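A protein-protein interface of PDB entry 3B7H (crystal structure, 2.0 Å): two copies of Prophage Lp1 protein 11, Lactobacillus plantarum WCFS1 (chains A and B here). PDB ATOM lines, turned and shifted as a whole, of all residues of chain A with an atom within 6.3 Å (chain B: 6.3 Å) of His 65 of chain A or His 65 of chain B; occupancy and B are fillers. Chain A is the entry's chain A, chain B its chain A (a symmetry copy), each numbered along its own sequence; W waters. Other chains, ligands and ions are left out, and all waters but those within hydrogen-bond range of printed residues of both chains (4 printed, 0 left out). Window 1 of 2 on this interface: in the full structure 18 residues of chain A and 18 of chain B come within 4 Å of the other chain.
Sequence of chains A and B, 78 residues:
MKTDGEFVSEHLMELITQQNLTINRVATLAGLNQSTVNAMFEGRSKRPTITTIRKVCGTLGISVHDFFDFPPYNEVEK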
ATOM      1  N   CYS A  57     -18.239  13.639  10.963  1.00  0.00           N
ATOM      2  CA  CYS A  57     -18.157  15.102  10.967  1.00  0.00           C
ATOM      3  C   CYS A  57     -16.850  15.553  10.353  1.00  0.00           C
ATOM      4  O   CYS A  57     -16.813  16.507   9.587  1.00  0.00           O
ATOM      5  CB  CYS A  57     -18.338  15.652  12.387  1.00  0.00           C
ATOM      6  SG  CYS A  57     -20.049  15.646  12.905  1.00  0.00           S
ATOM      7  N   SER A  63     -17.928  20.561  12.648  1.00  0.00           N
ATOM      8  CA  SER A  63     -17.690  20.234  14.061  1.00  0.00           C
ATOM      9  C   SER A  63     -18.889  19.448  14.586  1.00  0.00           C
ATOM     10  O   SER A  63     -20.001  19.612  14.080  1.00  0.00           O
ATOM     11  CB  SER A  63     -17.501  21.498  14.901  1.00  0.00           C
ATOM     12  OG  SER A  63     -18.716  22.201  15.093  1.00  0.00           O
ATOM     13  N   VAL A  64     -18.633  18.613  15.589  1.00  0.00           N
ATOM     14  CA  VAL A  64     -19.662  17.842  16.264  1.00  0.00           C
ATOM     15  C   VAL A  64     -20.666  18.789  16.898  1.00  0.00           C
ATOM     16  O   VAL A  64     -21.865  18.545  16.873  1.00  0.00           O
ATOM     17  CB  VAL A  64     -19.043  16.892  17.320  1.00  0.00           C
ATOM     18  CG1 VAL A  64     -20.087  16.389  18.336  1.00  0.00           C
ATOM     19  CG2 VAL A  64     -18.379  15.719  16.638  1.00  0.00           C
ATOM     20  N   HIS A  65     -20.177  19.879  17.463  1.00  0.00           N
ATOM     21  CA  HIS A  65     -21.038  20.941  17.975  1.00  0.00           C
ATOM     22  C   HIS A  65     -22.044  21.407  16.937  1.00  0.00           C
ATOM     23  O   HIS A  65     -23.245  21.476  17.222  1.00  0.00           O
ATOM     24  CB  HIS A  65     -20.162  22.097  18.437  1.00  0.00           C
ATOM     25  CG  HIS A  65     -20.911  23.291  18.907  1.00  0.00           C
ATOM     26  ND1 HIS A  65     -21.805  23.251  19.953  1.00  0.00           N
ATOM     27  CD2 HIS A  65     -20.838  24.580  18.527  1.00  0.00           C
ATOM     28  CE1 HIS A  65     -22.274  24.466  20.178  1.00  0.00           C
ATOM     29  NE2 HIS A  65     -21.708  25.290  19.321  1.00  0.00           N
ATOM     30  N   ASP A  66     -21.562  21.718  15.734  1.00  0.00           N
ATOM     31  CA  ASP A  66     -22.452  22.137  14.646  1.00  0.00           C
ATOM     32  C   ASP A  66     -23.380  21.023  14.153  1.00  0.00           C
ATOM     33  O   ASP A  66     -24.570  21.277  13.861  1.00  0.00           O
ATOM     34  CB  ASP A  66     -21.663  22.720  13.481  1.00  0.00           C
ATOM     35  CG  ASP A  66     -21.201  24.168  13.744  1.00  0.00           C
ATOM     36  OD1 ASP A  66     -21.751  24.850  14.645  1.00  0.00           O
ATOM     37  OD2 ASP A  66     -20.280  24.622  13.044  1.00  0.00           O
ATOM     38  N   PHE A  67     -22.856  19.800  14.096  1.00  0.00           N
ATOM     39  CA  PHE A  67     -23.683  18.629  13.803  1.00  0.00           C
ATOM     40  C   PHE A  67     -24.962  18.613  14.653  1.00  0.00           C
ATOM     41  O   PHE A  67     -26.039  18.328  14.155  1.00  0.00           O
ATOM     42  CB  PHE A  67     -22.899  17.325  14.018  1.00  0.00           C
ATOM     43  CG  PHE A  67     -23.728  16.096  13.777  1.00  0.00           C
ATOM     44  CD1 PHE A  67     -23.851  15.577  12.510  1.00  0.00           C
ATOM     45  CD2 PHE A  67     -24.455  15.530  14.801  1.00  0.00           C
ATOM     46  CE1 PHE A  67     -24.661  14.476  12.261  1.00  0.00           C
ATOM     47  CE2 PHE A  67     -25.279  14.437  14.573  1.00  0.00           C
ATOM     48  CZ  PHE A  67     -25.393  13.913  13.302  1.00  0.00           C
ATOM     49  N   PHE A  68     -24.848  18.956  15.922  1.00  0.00           N
ATOM     50  CA  PHE A  68     -25.956  18.840  16.836  1.00  0.00           C
ATOM     51  C   PHE A  68     -26.834  20.081  16.911  1.00  0.00           C
ATOM     52  O   PHE A  68     -27.692  20.156  17.795  1.00  0.00           O
ATOM     53  CB  PHE A  68     -25.454  18.467  18.232  1.00  0.00           C
ATOM     54  CG  PHE A  68     -25.207  16.985  18.420  1.00  0.00           C
ATOM     55  CD1 PHE A  68     -26.272  16.100  18.459  1.00  0.00           C
ATOM     56  CD2 PHE A  68     -23.923  16.491  18.570  1.00  0.00           C
ATOM     57  CE1 PHE A  68     -26.067  14.753  18.631  1.00  0.00           C
ATOM     58  CE2 PHE A  68     -23.717  15.127  18.742  1.00  0.00           C
ATOM     59  CZ  PHE A  68     -24.787  14.268  18.778  1.00  0.00           C
ATOM     60  N   ASP A  69     -26.652  21.035  15.994  1.00  0.00           N
ATOM     61  CA  ASP A  69     -27.470  22.234  15.949  1.00  0.00           C
ATOM     62  C   ASP A  69     -28.728  21.938  15.169  1.00  0.00           C
ATOM     63  O   ASP A  69     -28.952  22.507  14.093  1.00  0.00           O
ATOM     64  CB  ASP A  69     -26.680  23.385  15.321  1.00  0.00           C
ATOM     65  CG  ASP A  69     -27.350  24.751  15.478  1.00  0.00           C
ATOM     66  OD1 ASP A  69     -28.398  24.884  16.184  1.00  0.00           O
ATOM     67  OD2 ASP A  69     -26.788  25.716  14.870  1.00  0.00           O
ATOM     68  N   PHE A  70     -29.547  21.035  15.712  1.00  0.00           N
ATOM     69  CA  PHE A  70     -30.885  20.730  15.177  1.00  0.00           C
ATOM     70  C   PHE A  70     -31.717  20.158  16.288  1.00  0.00           C
ATOM     71  O   PHE A  70     -31.158  19.634  17.242  1.00  0.00           O
ATOM     72  CB  PHE A  70     -30.849  19.729  14.016  1.00  0.00           C
ATOM     73  CG  PHE A  70     -30.461  18.333  14.405  1.00  0.00           C
ATOM     74  CD1 PHE A  70     -31.409  17.342  14.496  1.00  0.00           C
ATOM     75  CD2 PHE A  70     -29.130  18.002  14.645  1.00  0.00           C
ATOM     76  CE1 PHE A  70     -31.064  16.051  14.837  1.00  0.00           C
ATOM     77  CE2 PHE A  70     -28.774  16.720  14.989  1.00  0.00           C
ATOM     78  CZ  PHE A  70     -29.736  15.732  15.065  1.00  0.00           C
ATOM     79  N   TYR A  73     -31.844  18.285  19.812  1.00  0.00           N
ATOM     80  CA  TYR A  73     -30.578  18.388  20.522  1.00  0.00           C
ATOM     81  C   TYR A  73     -30.143  19.827  20.799  1.00  0.00           C
ATOM     82  O   TYR A  73     -29.331  20.052  21.690  1.00  0.00           O
ATOM     83  CB  TYR A  73     -29.491  17.641  19.764  1.00  0.00           C
ATOM     84  CG  TYR A  73     -29.774  16.172  19.665  1.00  0.00           C
ATOM     85  CD1 TYR A  73     -30.163  15.616  18.470  1.00  0.00           C
ATOM     86  CD2 TYR A  73     -29.723  15.350  20.786  1.00  0.00           C
ATOM     87  CE1 TYR A  73     -30.442  14.243  18.366  1.00  0.00           C
ATOM     88  CE2 TYR A  73     -30.011  13.976  20.694  1.00  0.00           C
ATOM     89  CZ  TYR A  73     -30.357  13.436  19.476  1.00  0.00           C
ATOM     90  OH  TYR A  73     -30.657  12.093  19.333  1.00  0.00           O
ATOM     91  N   ASN A  74     -30.694  20.792  20.064  1.00  0.00           N
ATOM     92  CA  ASN A  74     -30.387  22.194  20.299  1.00  0.00           C
ATOM     93  C   ASN A  74     -31.458  22.926  21.078  1.00  0.00           C
ATOM     94  O   ASN A  74     -31.481  24.160  21.088  1.00  0.00           O
ATOM     95  CB  ASN A  74     -30.013  22.922  18.985  1.00  0.00           C
ATOM     96  CG  ASN A  74     -31.163  23.122  18.024  1.00  0.00           C
ATOM     97  OD1 ASN A  74     -32.295  22.649  18.231  1.00  0.00           O
ATOM     98  ND2 ASN A  74     -30.866  23.835  16.935  1.00  0.00           N
ATOM     99  N   GLU A  75     -32.335  22.185  21.737  1.00  0.00           N
ATOM    100  CA  GLU A  75     -33.259  22.786  22.693  1.00  0.00           C
ATOM    101  C   GLU A  75     -33.217  22.022  24.007  1.00  0.00           C
ATOM    102  O   GLU A  75     -32.796  20.876  24.009  1.00  0.00           O
ATOM    103  CB  GLU A  75     -34.661  22.789  22.090  1.00  0.00           C
ATOM    104  CG  GLU A  75     -34.772  23.660  20.773  1.00  0.00           C
ATOM    105  CD  GLU A  75     -34.622  25.224  20.961  1.00  0.00           C
ATOM    106  OE1 GLU A  75     -35.399  25.817  21.772  1.00  0.00           O
ATOM    107  OE2 GLU A  75     -33.759  25.866  20.261  1.00  0.00           O
ATOM    108  N   CYS B  57     -27.894  15.808  30.226  1.00  0.00           N
ATOM    109  CA  CYS B  57     -28.138  17.195  29.820  1.00  0.00           C
ATOM    110  C   CYS B  57     -29.496  17.650  30.306  1.00  0.00           C
ATOM    111  O   CYS B  57     -29.652  18.767  30.779  1.00  0.00           O
ATOM    112  CB  CYS B  57     -27.997  17.348  28.301  1.00  0.00           C
ATOM    113  SG  CYS B  57     -26.288  17.390  27.778  1.00  0.00           S
ATOM    114  N   SER B  63     -28.947  21.918  26.702  1.00  0.00           N
ATOM    115  CA  SER B  63     -29.124  21.189  25.438  1.00  0.00           C
ATOM    116  C   SER B  63     -27.837  20.427  25.132  1.00  0.00           C
ATOM    117  O   SER B  63     -26.758  20.848  25.555  1.00  0.00           O
ATOM    118  CB  SER B  63     -29.439  22.143  24.284  1.00  0.00           C
ATOM    119  OG  SER B  63     -28.307  22.896  23.887  1.00  0.00           O
ATOM    120  N   VAL B  64     -27.983  19.325  24.402  1.00  0.00           N
ATOM    121  CA  VAL B  64     -26.864  18.517  23.950  1.00  0.00           C
ATOM    122  C   VAL B  64     -25.962  19.358  23.063  1.00  0.00           C
ATOM    123  O   VAL B  64     -24.744  19.265  23.135  1.00  0.00           O
ATOM    124  CB  VAL B  64     -27.356  17.249  23.207  1.00  0.00           C
ATOM    125  CG1 VAL B  64     -26.248  16.605  22.353  1.00  0.00           C
ATOM    126  CG2 VAL B  64     -27.897  16.245  24.196  1.00  0.00           C
ATOM    127  N   HIS B  65     -26.561  20.188  22.227  1.00  0.00           N
ATOM    128  CA  HIS B  65     -25.815  21.156  21.428  1.00  0.00           C
ATOM    129  C   HIS B  65     -24.884  21.999  22.281  1.00  0.00           C
ATOM    130  O   HIS B  65     -23.693  22.120  21.970  1.00  0.00           O
ATOM    131  CB  HIS B  65     -26.806  22.035  20.680  1.00  0.00           C
ATOM    132  CG  HIS B  65     -26.188  23.129  19.886  1.00  0.00           C
ATOM    133  ND1 HIS B  65     -25.279  22.902  18.878  1.00  0.00           N
ATOM    134  CD2 HIS B  65     -26.410  24.456  19.897  1.00  0.00           C
ATOM    135  CE1 HIS B  65     -24.944  24.051  18.319  1.00  0.00           C
ATOM    136  NE2 HIS B  65     -25.612  25.012  18.924  1.00  0.00           N
ATOM    137  N   ASP B  66     -25.416  22.576  23.360  1.00  0.00           N
ATOM    138  CA  ASP B  66     -24.595  23.375  24.275  1.00  0.00           C
ATOM    139  C   ASP B  66     -23.556  22.550  25.042  1.00  0.00           C
ATOM    140  O   ASP B  66     -22.407  23.005  25.234  1.00  0.00           O
ATOM    141  CB  ASP B  66     -25.462  24.164  25.247  1.00  0.00           C
ATOM    142  CG  ASP B  66     -26.078  25.423  24.601  1.00  0.00           C
ATOM    143  OD1 ASP B  66     -25.593  25.887  23.539  1.00  0.00           O
ATOM    144  OD2 ASP B  66     -27.055  25.947  25.163  1.00  0.00           O
ATOM    145  N   PHE B  67     -23.942  21.340  25.442  1.00  0.00           N
ATOM    146  CA  PHE B  67     -22.995  20.395  26.034  1.00  0.00           C
ATOM    147  C   PHE B  67     -21.709  20.287  25.202  1.00  0.00           C
ATOM    148  O   PHE B  67     -20.615  20.272  25.742  1.00  0.00           O
ATOM    149  CB  PHE B  67     -23.625  19.003  26.200  1.00  0.00           C
ATOM    150  CG  PHE B  67     -22.669  17.988  26.757  1.00  0.00           C
ATOM    151  CD1 PHE B  67     -22.508  17.856  28.117  1.00  0.00           C
ATOM    152  CD2 PHE B  67     -21.867  17.247  25.918  1.00  0.00           C
ATOM    153  CE1 PHE B  67     -21.585  16.964  28.647  1.00  0.00           C
ATOM    154  CE2 PHE B  67     -20.930  16.358  26.426  1.00  0.00           C
ATOM    155  CZ  PHE B  67     -20.779  16.220  27.790  1.00  0.00           C
ATOM    156  N   PHE B  68     -21.840  20.252  23.890  1.00  0.00           N
ATOM    157  CA  PHE B  68     -20.713  20.012  23.025  1.00  0.00           C
ATOM    158  C   PHE B  68     -19.976  21.274  22.597  1.00  0.00           C
ATOM    159  O   PHE B  68     -19.119  21.198  21.713  1.00  0.00           O
ATOM    160  CB  PHE B  68     -21.148  19.215  21.795  1.00  0.00           C
ATOM    161  CG  PHE B  68     -21.225  17.721  22.027  1.00  0.00           C
ATOM    162  CD1 PHE B  68     -20.067  16.983  22.217  1.00  0.00           C
ATOM    163  CD2 PHE B  68     -22.444  17.065  22.039  1.00  0.00           C
ATOM    164  CE1 PHE B  68     -20.119  15.627  22.426  1.00  0.00           C
ATOM    165  CE2 PHE B  68     -22.494  15.692  22.253  1.00  0.00           C
ATOM    166  CZ  PHE B  68     -21.334  14.981  22.439  1.00  0.00           C
ATOM    167  N   ASP B  69     -20.278  22.417  23.218  1.00  0.00           N
ATOM    168  CA  ASP B  69     -19.599  23.666  22.918  1.00  0.00           C
ATOM    169  C   ASP B  69     -18.329  23.738  23.729  1.00  0.00           C
ATOM    170  O   ASP B  69     -18.186  24.603  24.602  1.00  0.00           O
ATOM    171  CB  ASP B  69     -20.522  24.850  23.216  1.00  0.00           C
ATOM    172  CG  ASP B  69     -20.006  26.186  22.678  1.00  0.00           C
ATOM    173  OD1 ASP B  69     -18.969  26.234  21.946  1.00  0.00           O
ATOM    174  OD2 ASP B  69     -20.682  27.212  23.004  1.00  0.00           O
ATOM    175  N   PHE B  70     -17.406  22.818  23.444  1.00  0.00           N
ATOM    176  CA  PHE B  70     -16.051  22.823  24.021  1.00  0.00           C
ATOM    177  C   PHE B  70     -15.143  22.063  23.098  1.00  0.00           C
ATOM    178  O   PHE B  70     -15.625  21.237  22.334  1.00  0.00           O
ATOM    179  CB  PHE B  70     -15.994  22.184  25.414  1.00  0.00           C
ATOM    180  CG  PHE B  70     -16.218  20.700  25.431  1.00  0.00           C
ATOM    181  CD1 PHE B  70     -15.164  19.834  25.602  1.00  0.00           C
ATOM    182  CD2 PHE B  70     -17.500  20.170  25.313  1.00  0.00           C
ATOM    183  CE1 PHE B  70     -15.357  18.470  25.636  1.00  0.00           C
ATOM    184  CE2 PHE B  70     -17.705  18.811  25.342  1.00  0.00           C
ATOM    185  CZ  PHE B  70     -16.638  17.954  25.525  1.00  0.00           C
ATOM    186  N   TYR B  73     -14.753  19.316  20.226  1.00  0.00           N
ATOM    187  CA  TYR B  73     -16.011  19.078  19.535  1.00  0.00           C
ATOM    188  C   TYR B  73     -16.600  20.327  18.879  1.00  0.00           C
ATOM    189  O   TYR B  73     -17.417  20.205  17.973  1.00  0.00           O
ATOM    190  CB  TYR B  73     -17.020  18.453  20.487  1.00  0.00           C
ATOM    191  CG  TYR B  73     -16.576  17.109  20.983  1.00  0.00           C
ATOM    192  CD1 TYR B  73     -16.147  16.951  22.279  1.00  0.00           C
ATOM    193  CD2 TYR B  73     -16.518  16.009  20.134  1.00  0.00           C
ATOM    194  CE1 TYR B  73     -15.719  15.700  22.753  1.00  0.00           C
ATOM    195  CE2 TYR B  73     -16.081  14.755  20.597  1.00  0.00           C
ATOM    196  CZ  TYR B  73     -15.696  14.615  21.911  1.00  0.00           C
ATOM    197  OH  TYR B  73     -15.251  13.405  22.414  1.00  0.00           O
ATOM    198  N   ASN B  74     -16.171  21.513  19.310  1.00  0.00           N
ATOM    199  CA  ASN B  74     -16.628  22.752  18.702  1.00  0.00           C
ATOM    200  C   ASN B  74     -15.633  23.355  17.735  1.00  0.00           C
ATOM    201  O   ASN B  74     -15.747  24.533  17.385  1.00  0.00           O
ATOM    202  CB  ASN B  74     -17.102  23.768  19.770  1.00  0.00           C
ATOM    203  CG  ASN B  74     -15.996  24.352  20.620  1.00  0.00           C
ATOM    204  OD1 ASN B  74     -14.815  23.970  20.534  1.00  0.00           O
ATOM    205  ND2 ASN B  74     -16.387  25.300  21.475  1.00  0.00           N
ATOM    206  N   GLU B  75     -14.669  22.563  17.292  1.00  0.00           N
ATOM    207  CA  GLU B  75     -13.802  22.977  16.193  1.00  0.00           C
ATOM    208  C   GLU B  75     -13.739  21.879  15.142  1.00  0.00           C
ATOM    209  O   GLU B  75     -14.030  20.738  15.463  1.00  0.00           O
ATOM    210  CB  GLU B  75     -12.420  23.301  16.749  1.00  0.00           C
ATOM    211  CG  GLU B  75     -12.426  24.509  17.774  1.00  0.00           C
ATOM    212  CD  GLU B  75     -12.746  25.933  17.164  1.00  0.00           C
ATOM    213  OE1 GLU B  75     -12.028  26.362  16.208  1.00  0.00           O
ATOM    214  OE2 GLU B  75     -13.687  26.643  17.673  1.00  0.00           O
HETATM  215  O   HOH W   1     -23.709  26.283  21.947  1.00  0.00           O
HETATM  216  O   HOH W   2     -15.707  18.354  16.033  1.00  0.00           O
HETATM  217  O   HOH W   3     -30.854  18.630  24.092  1.00  0.00           O
HETATM  218  O   HOH W   4     -23.693  25.458  16.096  1.00  0.00           O
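Of the printed residues of chain B, Asp 69 of chain A touches His 65 (3.5 Å).
Printed residues of chain B within 4 Å of Tyr 73 of chain A: Ser 63, Val 64 and His 65.
His 65 of chain B touches just these residues of chain A: His 65 (3.0 Å), Phe 68 (3.6 Å), Asp 69 (3.5 Å), Tyr 73 (2.8 Å) and Asn 74 (3.6 Å).
Of the printed residues of chain A, Glu 75 of chain B touches Ser 63.
The nearest residue of chain A that does not touch His 65 of chain B is Asp 66 of chain A (4.8 Å).
Val 64 of chain A touches Phe 68 of chain B, and with the chains exchanged Phe 68 of chain A touches Val 64 of chain B.
His 65 of chain A touches its own counterpart, His 65 of chain B.
His 65 of chain A touches Phe 68 of chain B, and with the chains exchanged Phe 68 of chain A touches His 65 of chain B.
Phe 68 of chain B touches its own counterpart, Phe 68 of chain A.
12 positions are printed for both chains.
The backbone NH (N) of Asp 66 of chain A lies within hydrogen-bond range of the side-chain hydroxyl (OG) of Ser 63 of chain A, 3.0 Å away.
The side-chain carboxylate (OD1) of Asp 69 of chain A sits at hydrogen-bond distance from the side-chain amide nitrogen (ND2) of Asn 74 of chain A.
ND2 of Asn 74 of chain A lies close to N of Phe 70 of chain A (3.3 Å).
OG of Ser 63 of chain B is in hydrogen-bond range of N of Asp 66 of chain B, 3.0 Å away.
The side-chain carboxylate (OD1) of Asp 69 of chain B sits at hydrogen-bond distance from the side-chain amide nitrogen (ND2) of Asn 74 of chain B (2.8 Å).
ND2 of Asn 74 of chain B sits close to N of Phe 70 of chain B (3.3 Å).
N of Val 64 of chain A sits at hydrogen-bond distance from O of Tyr 73 of chain B.
O of His 65 of chain A lies within hydrogen-bond range of ND1 of His 65 of chain B (3.0 Å).
The backbone carbonyl oxygen of Tyr 73 of chain B is in hydrogen-bond range of the backbone NH of His 65 of chain A, 2.8 Å away.
The backbone carbonyl oxygen (O) of Tyr 73 of chain A lies within hydrogen-bond range of the backbone NH (N) of Val 64 of chain B (3.1 Å).
The backbone NH of His 65 of chain B is in hydrogen-bond range of the backbone carbonyl oxygen of Tyr 73 of chain A (2.8 Å).
Water W4 lies within hydrogen-bond range of OD1 of Asp 66 of chain A (2.5 Å), OD2 of Asp 69 of chain A (3.3 Å) and NE2 of His 65 of chain B (3.4 Å).
Water W1 lies within hydrogen-bond range of the side-chain carboxylate of Asp 66 of chain B (2.5 Å), the side-chain carboxylate of Asp 69 of chain B (3.3 Å) and a ring nitrogen (NE2) of His 65 of chain A (3.4 Å).
Water W3 lies within hydrogen-bond range of O of Glu 75 of chain A (3.0 Å), N of Val 64 of chain B (3.0 Å) and O of Tyr 73 of chain A (3.2 Å).
Water W2 lies within hydrogen-bond range of O of Glu 75 of chain B (3.0 Å), N of Val 64 of chain A (3.0 Å) and O of Tyr 73 of chain B (3.2 Å).
Ser 63 of chain A touches Glu 75 of chain B (CB to O, 3.6 Å).
Val 64 of chain A touches Phe 68 of chain B.
CB of His 65 of chain A touches O of Phe 68 of chain B, 3.6 Å away.
His 65 of chain A touches Asp 69 of chain B.
Phe 68 of chain A touches Val 64 of chain B.
Phe 68 of chain A touches Phe 68 of chain B (CE2 to CE2, 3.8 Å).
His 65 of chain B touches Asp 69 of chain A.
Ser 63 of chain B touches Asn 74 of chain A.
Asn 74 of chain A touches His 65 of chain B (CA to CB, 3.6 Å).
O of Glu 75 of chain A touches CB of Ser 63 of chain B, at 3.6 Å.
Of the 12 printed residues of chain A, 8 touch a printed residue of chain B.
Printed residues of chain A that touch a printed residue of chain B: Ser 63, Val 64, His 65, Phe 68, Asp 69, Tyr 73, Asn 74 and Glu 75.
Printed residues of chain B that touch a printed residue of chain A: Ser 63, Val 64, His 65, Phe 68, Asp 69, Tyr 73, Asn 74 and Glu 75.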
